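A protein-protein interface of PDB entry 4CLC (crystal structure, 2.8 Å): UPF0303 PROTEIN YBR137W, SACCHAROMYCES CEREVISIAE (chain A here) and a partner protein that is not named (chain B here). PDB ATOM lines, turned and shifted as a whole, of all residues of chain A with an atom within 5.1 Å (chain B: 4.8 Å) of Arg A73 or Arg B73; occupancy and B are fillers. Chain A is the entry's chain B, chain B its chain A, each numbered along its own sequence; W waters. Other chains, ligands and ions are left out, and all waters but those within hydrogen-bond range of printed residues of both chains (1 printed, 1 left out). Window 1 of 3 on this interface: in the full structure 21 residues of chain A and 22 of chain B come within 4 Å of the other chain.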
ATOM      1  N   ALA A  60      -3.126   1.244 -10.646  1.00  0.00           N
ATOM      2  CA  ALA A  60      -2.130   0.245 -10.290  1.00  0.00           C
ATOM      3  C   ALA A  60      -0.846   0.922  -9.835  1.00  0.00           C
ATOM      4  O   ALA A  60      -0.367   1.850 -10.496  1.00  0.00           O
ATOM      5  CB  ALA A  60      -1.862  -0.674 -11.467  1.00  0.00           C
ATOM      6  N   ILE A  61      -0.296   0.475  -8.705  1.00  0.00           N
ATOM      7  CA  ILE A  61       0.971   1.020  -8.212  1.00  0.00           C
ATOM      8  C   ILE A  61       2.044  -0.055  -8.195  1.00  0.00           C
ATOM      9  O   ILE A  61       1.806  -1.182  -7.761  1.00  0.00           O
ATOM     10  CB  ILE A  61       0.840   1.627  -6.785  1.00  0.00           C
ATOM     11  CG1 ILE A  61      -0.190   2.761  -6.757  1.00  0.00           C
ATOM     12  CG2 ILE A  61       2.187   2.164  -6.300  1.00  0.00           C
ATOM     13  CD1 ILE A  61      -1.492   2.384  -6.125  1.00  0.00           C
ATOM     14  N   ASP A  62       3.231   0.299  -8.662  1.00  0.00           N
ATOM     15  CA  ASP A  62       4.324  -0.648  -8.729  1.00  0.00           C
ATOM     16  C   ASP A  62       5.638   0.032  -8.370  1.00  0.00           C
ATOM     17  O   ASP A  62       5.899   1.146  -8.826  1.00  0.00           O
ATOM     18  CB  ASP A  62       4.403  -1.250 -10.136  1.00  0.00           C
ATOM     19  CG  ASP A  62       5.504  -2.283 -10.272  1.00  0.00           C
ATOM     20  OD1 ASP A  62       5.216  -3.471  -9.995  1.00  0.00           O
ATOM     21  OD2 ASP A  62       6.648  -1.910 -10.656  1.00  0.00           O
ATOM     22  N   CYS A  70      10.484  -7.077  -8.998  1.00  0.00           N
ATOM     23  CA  CYS A  70       9.303  -6.355  -8.517  1.00  0.00           C
ATOM     24  C   CYS A  70       9.073  -6.481  -7.019  1.00  0.00           C
ATOM     25  O   CYS A  70       8.716  -7.547  -6.540  1.00  0.00           O
ATOM     26  CB  CYS A  70       8.060  -6.842  -9.239  1.00  0.00           C
ATOM     27  SG  CYS A  70       6.598  -6.064  -8.625  1.00  0.00           S
ATOM     28  N   LEU A  71       9.267  -5.379  -6.297  1.00  0.00           N
ATOM     29  CA  LEU A  71       9.162  -5.351  -4.844  1.00  0.00           C
ATOM     30  C   LEU A  71       7.729  -5.198  -4.338  1.00  0.00           C
ATOM     31  O   LEU A  71       7.366  -5.755  -3.299  1.00  0.00           O
ATOM     32  CB  LEU A  71      10.022  -4.224  -4.275  1.00  0.00           C
ATOM     33  CG  LEU A  71      11.525  -4.378  -4.512  1.00  0.00           C
ATOM     34  CD1 LEU A  71      12.350  -3.430  -3.634  1.00  0.00           C
ATOM     35  CD2 LEU A  71      11.967  -5.834  -4.352  1.00  0.00           C
ATOM     36  N   PHE A  72       6.934  -4.391  -5.035  1.00  0.00           N
ATOM     37  CA  PHE A  72       5.568  -4.121  -4.605  1.00  0.00           C
ATOM     38  C   PHE A  72       4.664  -3.894  -5.796  1.00  0.00           C
ATOM     39  O   PHE A  72       5.021  -3.179  -6.730  1.00  0.00           O
ATOM     40  CB  PHE A  72       5.534  -2.895  -3.678  1.00  0.00           C
ATOM     41  CG  PHE A  72       4.143  -2.397  -3.363  1.00  0.00           C
ATOM     42  CD1 PHE A  72       3.455  -2.878  -2.267  1.00  0.00           C
ATOM     43  CD2 PHE A  72       3.535  -1.430  -4.151  1.00  0.00           C
ATOM     44  CE1 PHE A  72       2.172  -2.418  -1.972  1.00  0.00           C
ATOM     45  CE2 PHE A  72       2.253  -0.980  -3.869  1.00  0.00           C
ATOM     46  CZ  PHE A  72       1.579  -1.470  -2.771  1.00  0.00           C
ATOM     47  N   ARG A  73       3.481  -4.482  -5.754  1.00  0.00           N
ATOM     48  CA  ARG A  73       2.461  -4.153  -6.730  1.00  0.00           C
ATOM     49  C   ARG A  73       1.099  -4.166  -6.077  1.00  0.00           C
ATOM     50  O   ARG A  73       0.764  -5.112  -5.348  1.00  0.00           O
ATOM     51  CB  ARG A  73       2.478  -5.137  -7.901  1.00  0.00           C
ATOM     52  CG  ARG A  73       1.265  -5.052  -8.829  1.00  0.00           C
ATOM     53  CD  ARG A  73       1.395  -3.887  -9.795  1.00  0.00           C
ATOM     54  NE  ARG A  73       2.640  -3.921 -10.581  1.00  0.00           N
ATOM     55  CZ  ARG A  73       2.812  -4.586 -11.729  1.00  0.00           C
ATOM     56  NH1 ARG A  73       1.822  -5.303 -12.258  1.00  0.00           N
ATOM     57  NH2 ARG A  73       3.984  -4.537 -12.349  1.00  0.00           N
ATOM     58  N   THR A  74       0.305  -3.132  -6.332  1.00  0.00           N
ATOM     59  CA  THR A  74      -1.092  -3.198  -5.924  1.00  0.00           C
ATOM     60  C   THR A  74      -2.049  -2.488  -6.886  1.00  0.00           C
ATOM     61  O   THR A  74      -1.630  -1.825  -7.841  1.00  0.00           O
ATOM     62  CB  THR A  74      -1.292  -2.599  -4.530  1.00  0.00           C
ATOM     63  OG1 THR A  74      -2.469  -3.158  -3.947  1.00  0.00           O
ATOM     64  CG2 THR A  74      -1.435  -1.084  -4.618  1.00  0.00           C
ATOM     65  N   VAL A  75      -3.340  -2.612  -6.595  1.00  0.00           N
ATOM     66  CA  VAL A  75      -4.375  -1.934  -7.353  1.00  0.00           C
ATOM     67  C   VAL A  75      -5.490  -1.467  -6.391  1.00  0.00           C
ATOM     68  O   VAL A  75      -5.802  -2.156  -5.411  1.00  0.00           O
ATOM     69  CB  VAL A  75      -4.921  -2.852  -8.484  1.00  0.00           C
ATOM     70  CG1 VAL A  75      -5.178  -4.259  -7.973  1.00  0.00           C
ATOM     71  CG2 VAL A  75      -6.165  -2.261  -9.080  1.00  0.00           C
ATOM     72  N   ASP A  85      -0.847  -3.660 -16.272  1.00  0.00           N
ATOM     73  CA  ASP A  85       0.455  -4.329 -16.349  1.00  0.00           C
ATOM     74  C   ASP A  85       1.302  -3.853 -17.544  1.00  0.00           C
ATOM     75  O   ASP A  85       2.490  -3.535 -17.394  1.00  0.00           O
ATOM     76  CB  ASP A  85       0.285  -5.844 -16.462  1.00  0.00           C
ATOM     77  CG  ASP A  85      -0.132  -6.502 -15.162  1.00  0.00           C
ATOM     78  OD1 ASP A  85      -1.296  -6.333 -14.727  1.00  0.00           O
ATOM     79  OD2 ASP A  85       0.709  -7.235 -14.600  1.00  0.00           O
ATOM     80  N   ILE A  88       2.384  -0.145 -16.940  1.00  0.00           N
ATOM     81  CA  ILE A  88       3.432  -0.107 -15.952  1.00  0.00           C
ATOM     82  C   ILE A  88       4.744  -0.551 -16.578  1.00  0.00           C
ATOM     83  O   ILE A  88       5.741   0.176 -16.540  1.00  0.00           O
ATOM     84  CB  ILE A  88       3.090  -0.978 -14.757  1.00  0.00           C
ATOM     85  CG1 ILE A  88       2.045  -0.263 -13.894  1.00  0.00           C
ATOM     86  CG2 ILE A  88       4.357  -1.274 -13.941  1.00  0.00           C
ATOM     87  CD1 ILE A  88       1.405  -1.136 -12.854  1.00  0.00           C
ATOM     88  N   ILE B  61       5.515 -12.854  -2.561  1.00  0.00           N
ATOM     89  CA  ILE B  61       4.136 -13.306  -2.520  1.00  0.00           C
ATOM     90  C   ILE B  61       3.366 -12.617  -3.635  1.00  0.00           C
ATOM     91  O   ILE B  61       3.457 -11.385  -3.792  1.00  0.00           O
ATOM     92  CB  ILE B  61       3.459 -12.979  -1.160  1.00  0.00           C
ATOM     93  CG1 ILE B  61       4.326 -13.434   0.010  1.00  0.00           C
ATOM     94  CG2 ILE B  61       2.063 -13.601  -1.064  1.00  0.00           C
ATOM     95  CD1 ILE B  61       3.619 -13.319   1.345  1.00  0.00           C
ATOM     96  N   ASP B  62       2.587 -13.396  -4.383  1.00  0.00           N
ATOM     97  CA  ASP B  62       1.865 -12.864  -5.532  1.00  0.00           C
ATOM     98  C   ASP B  62       0.435 -13.355  -5.647  1.00  0.00           C
ATOM     99  O   ASP B  62       0.171 -14.556  -5.553  1.00  0.00           O
ATOM    100  CB  ASP B  62       2.605 -13.220  -6.818  1.00  0.00           C
ATOM    101  CG  ASP B  62       1.963 -12.608  -8.044  1.00  0.00           C
ATOM    102  OD1 ASP B  62       2.186 -11.400  -8.295  1.00  0.00           O
ATOM    103  OD2 ASP B  62       1.229 -13.339  -8.749  1.00  0.00           O
ATOM    104  N   CYS B  70      -1.887  -8.794 -12.500  1.00  0.00           N
ATOM    105  CA  CYS B  70      -1.343  -8.921 -11.157  1.00  0.00           C
ATOM    106  C   CYS B  70      -1.990  -7.954 -10.160  1.00  0.00           C
ATOM    107  O   CYS B  70      -1.812  -6.741 -10.258  1.00  0.00           O
ATOM    108  CB  CYS B  70       0.164  -8.690 -11.199  1.00  0.00           C
ATOM    109  SG  CYS B  70       1.023  -9.029  -9.666  1.00  0.00           S
ATOM    110  N   LEU B  71      -2.742  -8.512  -9.211  1.00  0.00           N
ATOM    111  CA  LEU B  71      -3.393  -7.751  -8.141  1.00  0.00           C
ATOM    112  C   LEU B  71      -2.504  -7.418  -6.930  1.00  0.00           C
ATOM    113  O   LEU B  71      -2.563  -6.306  -6.387  1.00  0.00           O
ATOM    114  CB  LEU B  71      -4.609  -8.516  -7.654  1.00  0.00           C
ATOM    115  CG  LEU B  71      -5.590  -8.888  -8.759  1.00  0.00           C
ATOM    116  CD1 LEU B  71      -6.618  -9.835  -8.181  1.00  0.00           C
ATOM    117  CD2 LEU B  71      -6.253  -7.649  -9.342  1.00  0.00           C
ATOM    118  N   PHE B  72      -1.704  -8.387  -6.490  1.00  0.00           N
ATOM    119  CA  PHE B  72      -0.835  -8.164  -5.343  1.00  0.00           C
ATOM    120  C   PHE B  72       0.565  -8.740  -5.542  1.00  0.00           C
ATOM    121  O   PHE B  72       0.726  -9.881  -6.015  1.00  0.00           O
ATOM    122  CB  PHE B  72      -1.454  -8.757  -4.066  1.00  0.00           C
ATOM    123  CG  PHE B  72      -0.696  -8.400  -2.810  1.00  0.00           C
ATOM    124  CD1 PHE B  72      -0.994  -7.239  -2.108  1.00  0.00           C
ATOM    125  CD2 PHE B  72       0.333  -9.205  -2.351  1.00  0.00           C
ATOM    126  CE1 PHE B  72      -0.292  -6.903  -0.964  1.00  0.00           C
ATOM    127  CE2 PHE B  72       1.044  -8.871  -1.206  1.00  0.00           C
ATOM    128  CZ  PHE B  72       0.732  -7.719  -0.515  1.00  0.00           C
ATOM    129  N   ARG B  73       1.569  -7.936  -5.181  1.00  0.00           N
ATOM    130  CA  ARG B  73       2.950  -8.406  -5.094  1.00  0.00           C
ATOM    131  C   ARG B  73       3.710  -7.735  -3.957  1.00  0.00           C
ATOM    132  O   ARG B  73       3.674  -6.518  -3.826  1.00  0.00           O
ATOM    133  CB  ARG B  73       3.698  -8.151  -6.403  1.00  0.00           C
ATOM    134  CG  ARG B  73       5.180  -8.505  -6.337  1.00  0.00           C
ATOM    135  CD  ARG B  73       5.362  -9.997  -6.309  1.00  0.00           C
ATOM    136  NE  ARG B  73       4.734 -10.600  -7.479  1.00  0.00           N
ATOM    137  CZ  ARG B  73       5.366 -10.874  -8.613  1.00  0.00           C
ATOM    138  NH1 ARG B  73       6.662 -10.620  -8.732  1.00  0.00           N
ATOM    139  NH2 ARG B  73       4.701 -11.408  -9.624  1.00  0.00           N
ATOM    140  N   THR B  74       4.432  -8.522  -3.166  1.00  0.00           N
ATOM    141  CA  THR B  74       5.319  -7.962  -2.158  1.00  0.00           C
ATOM    142  C   THR B  74       6.447  -8.923  -1.807  1.00  0.00           C
ATOM    143  O   THR B  74       6.402 -10.111  -2.137  1.00  0.00           O
ATOM    144  CB  THR B  74       4.568  -7.604  -0.876  1.00  0.00           C
ATOM    145  OG1 THR B  74       5.352  -6.686  -0.102  1.00  0.00           O
ATOM    146  CG2 THR B  74       4.297  -8.854  -0.080  1.00  0.00           C
ATOM    147  N   VAL B  75       7.473  -8.390  -1.157  1.00  0.00           N
ATOM    148  CA  VAL B  75       8.560  -9.201  -0.628  1.00  0.00           C
ATOM    149  C   VAL B  75       8.635  -9.002   0.894  1.00  0.00           C
ATOM    150  O   VAL B  75       8.402  -7.897   1.399  1.00  0.00           O
ATOM    151  CB  VAL B  75       9.921  -8.856  -1.301  1.00  0.00           C
ATOM    152  CG1 VAL B  75      10.000  -9.461  -2.681  1.00  0.00           C
ATOM    153  CG2 VAL B  75      10.138  -7.355  -1.363  1.00  0.00           C
ATOM    154  N   ASP B  85      10.955 -13.653  -8.969  1.00  0.00           N
ATOM    155  CA  ASP B  85       9.969 -13.310  -9.984  1.00  0.00           C
ATOM    156  C   ASP B  85       9.846 -14.424 -11.013  1.00  0.00           C
ATOM    157  O   ASP B  85       8.749 -14.821 -11.413  1.00  0.00           O
ATOM    158  CB  ASP B  85      10.340 -11.992 -10.653  1.00  0.00           C
ATOM    159  CG  ASP B  85      10.207 -10.808  -9.714  1.00  0.00           C
ATOM    160  OD1 ASP B  85      10.077 -11.052  -8.501  1.00  0.00           O
ATOM    161  OD2 ASP B  85      10.225  -9.644 -10.185  1.00  0.00           O
ATOM    162  N   ILE B  88       7.852 -17.177  -9.299  1.00  0.00           N
ATOM    163  CA  ILE B  88       6.451 -16.805  -9.281  1.00  0.00           C
ATOM    164  C   ILE B  88       5.784 -17.062 -10.646  1.00  0.00           C
ATOM    165  O   ILE B  88       4.657 -17.526 -10.709  1.00  0.00           O
ATOM    166  CB  ILE B  88       6.276 -15.334  -8.902  1.00  0.00           C
ATOM    167  CG1 ILE B  88       6.752 -15.099  -7.467  1.00  0.00           C
ATOM    168  CG2 ILE B  88       4.822 -14.911  -9.095  1.00  0.00           C
ATOM    169  CD1 ILE B  88       6.386 -13.731  -6.884  1.00  0.00           C
ATOM    170  N   GLN B  89       6.495 -16.769 -11.734  1.00  0.00           N
ATOM    171  CA  GLN B  89       5.945 -16.937 -13.072  1.00  0.00           C
ATOM    172  C   GLN B  89       5.805 -18.402 -13.414  1.00  0.00           C
ATOM    173  O   GLN B  89       4.752 -18.847 -13.869  1.00  0.00           O
ATOM    174  CB  GLN B  89       6.822 -16.241 -14.119  1.00  0.00           C
ATOM    175  CG  GLN B  89       6.741 -14.738 -14.062  1.00  0.00           C
ATOM    176  CD  GLN B  89       5.342 -14.214 -14.371  1.00  0.00           C
ATOM    177  OE1 GLN B  89       4.864 -14.316 -15.508  1.00  0.00           O
ATOM    178  NE2 GLN B  89       4.680 -13.655 -13.360  1.00  0.00           N
HETATM  179  O   HOH W   1      -0.747  -4.753 -12.328  1.00  0.00           O
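Ala A60 touches none of the printed residues of chain B.
Asp A62 touches none of the printed residues of chain B.
Printed residues of chain B within 4 Å of Leu A71: Arg B73, Thr B74 and Val B75.
Of the printed residues of chain A, Cys B70 touches Arg A73 and Asp A85.
Of chain A, only Cys A70 (3.6 Å), Leu A71 (3.8 Å), Phe A72 (3.2 Å) and Arg A73 (2.8 Å) come within 4 Å of Arg B73.
The nearest printed residue of chain B that does not touch Arg A73 is Thr B74 (4.9 Å).
The nearest printed residue of chain A that does not touch Arg B73 is Thr A74 (5.1 Å).
The nearest printed residue of chain A that does not touch Val B75 is Cys A70 (4.5 Å).
Arg B73 touches Cys A70 (CG to SG, 3.6 Å).
O of Leu A71 touches O of Arg B73, 3.8 Å away.
Leu A71 touches Thr B74.
Phe A72 touches Arg B73 (CA to O, 3.2 Å).
Arg A73 touches Cys B70 (CG to O, 3.8 Å).
Arg A73 touches Leu B71.
Phe B72 touches Arg A73.
Thr A74 touches Leu B71 (CA to O, 3.5 Å).
CG1 of Val A75 touches O of Leu B71, 3.7 Å away.
The backbone NH (N) of Arg A73 sits at hydrogen-bond distance from the backbone carbonyl oxygen (O) of Arg B73, 2.8 Å away.
The backbone NH (N) of Cys B70 sits at hydrogen-bond distance from the side-chain carboxylate (OD1) of Asp A85, at 3.4 Å.
The backbone carbonyl oxygen of Leu A71 is in hydrogen-bond range of the backbone NH of Val B75, at 3.4 Å.
The side-chain carboxylate (OD2) of Asp B85 lies within hydrogen-bond range of the backbone NH (N) of Cys A70 (2.8 Å).
Water W1 lies within hydrogen-bond range of NH1 of Arg A73 (2.6 Å), OD1 of Asp A85 (2.9 Å) and O of Cys B70 (3.1 Å).
The side-chain carboxylate (OD1) of Asp B62 lies within salt-bridge range of the guanidinium group (NE) of Arg B73 (2.8 Å).
The side-chain carboxylate (OD1) of Asp A62 is in hydrogen-bond range of the side-chain sulfur (SG) of Cys A70, at 3.2 Å.
The guanidinium group of Arg A73 lies within salt-bridge range of the side-chain carboxylate of Asp A85 (3.2 Å).
The backbone carbonyl oxygen (O) of Phe A72 is in hydrogen-bond range of the side-chain sulfur (SG) of Cys A70 (3.8 Å).
The side-chain sulfur (SG) of Cys B70 sits at hydrogen-bond distance from the side-chain carboxylate (OD1) of Asp B62 (3.0 Å).
O of Thr B74 sits at hydrogen-bond distance from N of Ile B61 (2.9 Å).
Printed residues of chain B that touch a printed residue of chain A: Cys B70, Leu B71, Phe B72, Arg B73, Thr B74, Val B75 and Asp B85.
Hydrophobic or aromatic side chains of chain B within 4 Å of the printed part of chain A: Leu B71 and Val B75.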
